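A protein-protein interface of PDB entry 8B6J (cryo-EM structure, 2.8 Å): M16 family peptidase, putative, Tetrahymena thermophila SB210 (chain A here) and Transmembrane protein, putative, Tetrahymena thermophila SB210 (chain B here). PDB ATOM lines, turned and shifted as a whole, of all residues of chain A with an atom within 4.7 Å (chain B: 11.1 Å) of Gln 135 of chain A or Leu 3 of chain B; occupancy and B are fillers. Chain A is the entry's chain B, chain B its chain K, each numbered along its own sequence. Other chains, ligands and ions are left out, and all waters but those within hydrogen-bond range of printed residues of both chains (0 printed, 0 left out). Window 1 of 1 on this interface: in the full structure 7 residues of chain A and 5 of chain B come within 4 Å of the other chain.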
ATOM      1  N   GLY A 131      -4.599   7.524 -19.144  1.00  0.00           N
ATOM      2  CA  GLY A 131      -5.015   8.717 -18.426  1.00  0.00           C
ATOM      3  C   GLY A 131      -5.357   8.430 -16.978  1.00  0.00           C
ATOM      4  O   GLY A 131      -5.118   9.258 -16.100  1.00  0.00           O
ATOM      5  N   VAL A 132      -5.934   7.258 -16.713  1.00  0.00           N
ATOM      6  CA  VAL A 132      -6.196   6.851 -15.334  1.00  0.00           C
ATOM      7  C   VAL A 132      -4.890   6.764 -14.558  1.00  0.00           C
ATOM      8  O   VAL A 132      -4.772   7.280 -13.441  1.00  0.00           O
ATOM      9  CB  VAL A 132      -6.958   5.513 -15.306  1.00  0.00           C
ATOM     10  CG1 VAL A 132      -6.869   4.874 -13.932  1.00  0.00           C
ATOM     11  CG2 VAL A 132      -8.407   5.720 -15.700  1.00  0.00           C
ATOM     12  N   VAL A 133      -3.883   6.117 -15.149  1.00  0.00           N
ATOM     13  CA  VAL A 133      -2.576   6.031 -14.498  1.00  0.00           C
ATOM     14  C   VAL A 133      -2.021   7.426 -14.246  1.00  0.00           C
ATOM     15  O   VAL A 133      -1.531   7.735 -13.153  1.00  0.00           O
ATOM     16  CB  VAL A 133      -1.602   5.194 -15.347  1.00  0.00           C
ATOM     17  CG1 VAL A 133      -0.200   5.257 -14.764  1.00  0.00           C
ATOM     18  CG2 VAL A 133      -2.068   3.763 -15.439  1.00  0.00           C
ATOM     19  N   GLN A 134      -2.087   8.289 -15.259  1.00  0.00           N
ATOM     20  CA  GLN A 134      -1.484   9.614 -15.157  1.00  0.00           C
ATOM     21  C   GLN A 134      -2.174  10.465 -14.098  1.00  0.00           C
ATOM     22  O   GLN A 134      -1.507  11.157 -13.320  1.00  0.00           O
ATOM     23  CB  GLN A 134      -1.535  10.305 -16.517  1.00  0.00           C
ATOM     24  CG  GLN A 134      -0.803  11.625 -16.572  1.00  0.00           C
ATOM     25  CD  GLN A 134      -0.864  12.263 -17.942  1.00  0.00           C
ATOM     26  OE1 GLN A 134      -1.792  12.019 -18.710  1.00  0.00           O
ATOM     27  NE2 GLN A 134       0.129  13.083 -18.258  1.00  0.00           N
ATOM     28  N   GLN A 135      -3.506  10.432 -14.052  1.00  0.00           N
ATOM     29  CA  GLN A 135      -4.252  11.315 -13.166  1.00  0.00           C
ATOM     30  C   GLN A 135      -4.334  10.780 -11.745  1.00  0.00           C
ATOM     31  O   GLN A 135      -4.449  11.568 -10.802  1.00  0.00           O
ATOM     32  CB  GLN A 135      -5.659  11.538 -13.719  1.00  0.00           C
ATOM     33  CG  GLN A 135      -5.699  12.459 -14.920  1.00  0.00           C
ATOM     34  CD  GLN A 135      -5.464  13.906 -14.548  1.00  0.00           C
ATOM     35  OE1 GLN A 135      -5.788  14.334 -13.442  1.00  0.00           O
ATOM     36  NE2 GLN A 135      -4.892  14.667 -15.469  1.00  0.00           N
ATOM     37  N   SER A 136      -4.282   9.460 -11.564  1.00  0.00           N
ATOM     38  CA  SER A 136      -4.267   8.920 -10.211  1.00  0.00           C
ATOM     39  C   SER A 136      -3.035   9.366  -9.441  1.00  0.00           C
ATOM     40  O   SER A 136      -3.043   9.330  -8.206  1.00  0.00           O
ATOM     41  CB  SER A 136      -4.323   7.393 -10.251  1.00  0.00           C
ATOM     42  OG  SER A 136      -3.141   6.859 -10.817  1.00  0.00           O
ATOM     43  N   GLY A 137      -1.982   9.785 -10.140  1.00  0.00           N
ATOM     44  CA  GLY A 137      -0.747  10.189  -9.510  1.00  0.00           C
ATOM     45  C   GLY A 137       0.183   9.052  -9.168  1.00  0.00           C
ATOM     46  O   GLY A 137       1.346   9.305  -8.831  1.00  0.00           O
ATOM     47  N   MET B   1     -10.631  10.622  -9.706  1.00  0.00           N
ATOM     48  CA  MET B   1      -9.592  11.256 -10.564  1.00  0.00           C
ATOM     49  C   MET B   1     -10.236  12.140 -11.627  1.00  0.00           C
ATOM     50  O   MET B   1     -11.368  11.905 -12.044  1.00  0.00           O
ATOM     51  CB  MET B   1      -8.718  10.188 -11.219  1.00  0.00           C
ATOM     52  CG  MET B   1      -9.490   9.192 -12.061  1.00  0.00           C
ATOM     53  SD  MET B   1      -8.487   7.784 -12.559  1.00  0.00           S
ATOM     54  CE  MET B   1      -8.186   7.004 -10.977  1.00  0.00           C
ATOM     55  N   TYR B   2      -9.499  13.159 -12.056  1.00  0.00           N
ATOM     56  CA  TYR B   2      -9.999  14.155 -12.997  1.00  0.00           C
ATOM     57  C   TYR B   2      -9.613  13.725 -14.408  1.00  0.00           C
ATOM     58  O   TYR B   2      -8.439  13.794 -14.783  1.00  0.00           O
ATOM     59  CB  TYR B   2      -9.425  15.525 -12.650  1.00  0.00           C
ATOM     60  CG  TYR B   2     -10.106  16.696 -13.316  1.00  0.00           C
ATOM     61  CD1 TYR B   2     -11.374  17.098 -12.928  1.00  0.00           C
ATOM     62  CD2 TYR B   2      -9.465  17.421 -14.309  1.00  0.00           C
ATOM     63  CE1 TYR B   2     -11.994  18.174 -13.525  1.00  0.00           C
ATOM     64  CE2 TYR B   2     -10.077  18.496 -14.913  1.00  0.00           C
ATOM     65  CZ  TYR B   2     -11.340  18.870 -14.517  1.00  0.00           C
ATOM     66  OH  TYR B   2     -11.953  19.944 -15.115  1.00  0.00           O
ATOM     67  N   LEU B   3     -10.599  13.294 -15.193  1.00  0.00           N
ATOM     68  CA  LEU B   3     -10.371  12.741 -16.529  1.00  0.00           C
ATOM     69  C   LEU B   3     -11.245  13.479 -17.534  1.00  0.00           C
ATOM     70  O   LEU B   3     -12.172  12.905 -18.116  1.00  0.00           O
ATOM     71  CB  LEU B   3     -10.660  11.240 -16.555  1.00  0.00           C
ATOM     72  CG  LEU B   3      -9.628  10.346 -15.867  1.00  0.00           C
ATOM     73  CD1 LEU B   3     -10.150   8.930 -15.728  1.00  0.00           C
ATOM     74  CD2 LEU B   3      -8.320  10.348 -16.639  1.00  0.00           C
ATOM     75  N   PRO B   4     -10.967  14.758 -17.768  1.00  0.00           N
ATOM     76  CA  PRO B   4     -11.776  15.524 -18.717  1.00  0.00           C
ATOM     77  C   PRO B   4     -11.572  15.050 -20.145  1.00  0.00           C
ATOM     78  O   PRO B   4     -10.502  14.568 -20.522  1.00  0.00           O
ATOM     79  CB  PRO B   4     -11.270  16.958 -18.530  1.00  0.00           C
ATOM     80  CG  PRO B   4      -9.875  16.799 -18.061  1.00  0.00           C
ATOM     81  CD  PRO B   4      -9.858  15.553 -17.221  1.00  0.00           C
ATOM     82  N   THR B   5     -12.625  15.192 -20.943  1.00  0.00           N
ATOM     83  CA  THR B   5     -12.543  14.852 -22.354  1.00  0.00           C
ATOM     84  C   THR B   5     -11.657  15.854 -23.085  1.00  0.00           C
ATOM     85  O   THR B   5     -11.599  17.035 -22.738  1.00  0.00           O
ATOM     86  CB  THR B   5     -13.936  14.831 -22.980  1.00  0.00           C
ATOM     87  OG1 THR B   5     -14.834  14.112 -22.127  1.00  0.00           O
ATOM     88  CG2 THR B   5     -13.899  14.156 -24.339  1.00  0.00           C
ATOM     89  N   PHE B   6     -10.955  15.367 -24.108  1.00  0.00           N
ATOM     90  CA  PHE B   6     -10.079  16.243 -24.875  1.00  0.00           C
ATOM     91  C   PHE B   6     -10.861  17.290 -25.657  1.00  0.00           C
ATOM     92  O   PHE B   6     -10.303  18.344 -25.988  1.00  0.00           O
ATOM     93  CB  PHE B   6      -9.203  15.410 -25.808  1.00  0.00           C
ATOM     94  CG  PHE B   6      -8.353  14.406 -25.084  1.00  0.00           C
ATOM     95  CD1 PHE B   6      -7.287  14.818 -24.305  1.00  0.00           C
ATOM     96  CD2 PHE B   6      -8.626  13.055 -25.170  1.00  0.00           C
ATOM     97  CE1 PHE B   6      -6.511  13.901 -23.632  1.00  0.00           C
ATOM     98  CE2 PHE B   6      -7.853  12.135 -24.497  1.00  0.00           C
ATOM     99  CZ  PHE B   6      -6.796  12.558 -23.728  1.00  0.00           C
ATOM    100  N   TYR B   7     -12.139  17.034 -25.943  1.00  0.00           N
ATOM    101  CA  TYR B   7     -13.002  18.087 -26.467  1.00  0.00           C
ATOM    102  C   TYR B   7     -12.987  19.297 -25.544  1.00  0.00           C
ATOM    103  O   TYR B   7     -12.802  20.434 -25.989  1.00  0.00           O
ATOM    104  CB  TYR B   7     -14.434  17.572 -26.619  1.00  0.00           C
ATOM    105  CG  TYR B   7     -14.655  16.589 -27.742  1.00  0.00           C
ATOM    106  CD1 TYR B   7     -14.497  16.971 -29.065  1.00  0.00           C
ATOM    107  CD2 TYR B   7     -15.056  15.289 -27.480  1.00  0.00           C
ATOM    108  CE1 TYR B   7     -14.711  16.079 -30.093  1.00  0.00           C
ATOM    109  CE2 TYR B   7     -15.273  14.391 -28.501  1.00  0.00           C
ATOM    110  CZ  TYR B   7     -15.100  14.791 -29.805  1.00  0.00           C
ATOM    111  OH  TYR B   7     -15.317  13.898 -30.825  1.00  0.00           O
ATOM    112  N   LYS B   8     -13.188  19.062 -24.245  1.00  0.00           N
ATOM    113  CA  LYS B   8     -13.242  20.166 -23.296  1.00  0.00           C
ATOM    114  C   LYS B   8     -11.900  20.877 -23.193  1.00  0.00           C
ATOM    115  O   LYS B   8     -11.852  22.108 -23.098  1.00  0.00           O
ATOM    116  CB  LYS B   8     -13.681  19.659 -21.925  1.00  0.00           C
ATOM    117  CG  LYS B   8     -13.801  20.762 -20.890  1.00  0.00           C
ATOM    118  CD  LYS B   8     -14.411  20.266 -19.600  1.00  0.00           C
ATOM    119  CE  LYS B   8     -13.477  19.323 -18.881  1.00  0.00           C
ATOM    120  NZ  LYS B   8     -13.977  18.998 -17.525  1.00  0.00           N
ATOM    121  N   LEU B   9     -10.798  20.123 -23.186  1.00  0.00           N
ATOM    122  CA  LEU B   9      -9.487  20.757 -23.120  1.00  0.00           C
ATOM    123  C   LEU B   9      -9.255  21.647 -24.332  1.00  0.00           C
ATOM    124  O   LEU B   9      -8.779  22.783 -24.199  1.00  0.00           O
ATOM    125  CB  LEU B   9      -8.393  19.694 -23.023  1.00  0.00           C
ATOM    126  CG  LEU B   9      -8.535  18.683 -21.885  1.00  0.00           C
ATOM    127  CD1 LEU B   9      -7.336  17.750 -21.857  1.00  0.00           C
ATOM    128  CD2 LEU B   9      -8.701  19.382 -20.547  1.00  0.00           C
ATOM    129  N   GLU B  12     -11.443  24.829 -23.977  1.00  0.00           N
ATOM    130  CA  GLU B  12     -10.937  25.781 -22.993  1.00  0.00           C
ATOM    131  C   GLU B  12      -9.669  26.469 -23.484  1.00  0.00           C
ATOM    132  O   GLU B  12      -9.501  27.682 -23.300  1.00  0.00           O
ATOM    133  CB  GLU B  12     -10.685  25.066 -21.667  1.00  0.00           C
ATOM    134  CG  GLU B  12     -11.942  24.494 -21.032  1.00  0.00           C
ATOM    135  CD  GLU B  12     -11.641  23.590 -19.854  1.00  0.00           C
ATOM    136  OE1 GLU B  12     -10.453  23.290 -19.618  1.00  0.00           O
ATOM    137  OE2 GLU B  12     -12.595  23.178 -19.162  1.00  0.00           O
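Gln 135 of chain A touches just these residues of chain B: Tyr 2 (3.0 Å) and Leu 3 (3.8 Å).
Of chain A, only Gly 131 (3.4 Å), Val 132 (3.7 Å) and Gln 135 (3.8 Å) come within 4 Å of Leu 3 of chain B.
Val 133 of chain A touches none of the printed residues of chain B.
Ser 136 of chain A touches one residue of chain B.
Of the printed residues of chain A, Met 1 of chain B touches Val 132 and Ser 136.
Of the printed residues of chain A, Tyr 2 of chain B touches Gln 135.
Lys 8 of chain B touches none of the printed residues of chain A.
Gly 131 of chain A touches Leu 3 of chain B.
Met 1 of chain B touches Val 132 of chain A (SD to CG1, 3.6 Å).
Val 132 of chain A touches Leu 3 of chain B (CG2 to CD1, 3.7 Å).
Leu 3 of chain B touches Gln 135 of chain A (CD2 to CG, 3.8 Å).
Met 1 of chain B touches Ser 136 of chain A (CE to CB, 3.9 Å).
Of the 10 printed residues of chain B, 3 touch a printed residue of chain A.
Hydrophobic or aromatic side chains of chain B within 4 Å of the printed part of chain A: Met 1, Tyr 2 and Leu 3.
Among the printed residues, 6 pairs touch across the chains.
The side-chain amide oxygen (OE1) of Gln 135 of chain A sits close to the backbone carbonyl oxygen (O) of Tyr 2 of chain B, 3.0 Å away.
NZ of Lys 8 of chain B lies within hydrogen-bond range of OH of Tyr 2 of chain B, at 3.3 Å.
The backbone carbonyl oxygen of Val 133 of chain A lies within hydrogen-bond range of the side-chain hydroxyl of Ser 136 of chain A (3.0 Å).
O of Val 132 of chain A lies within hydrogen-bond range of OG of Ser 136 of chain A (3.1 Å).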
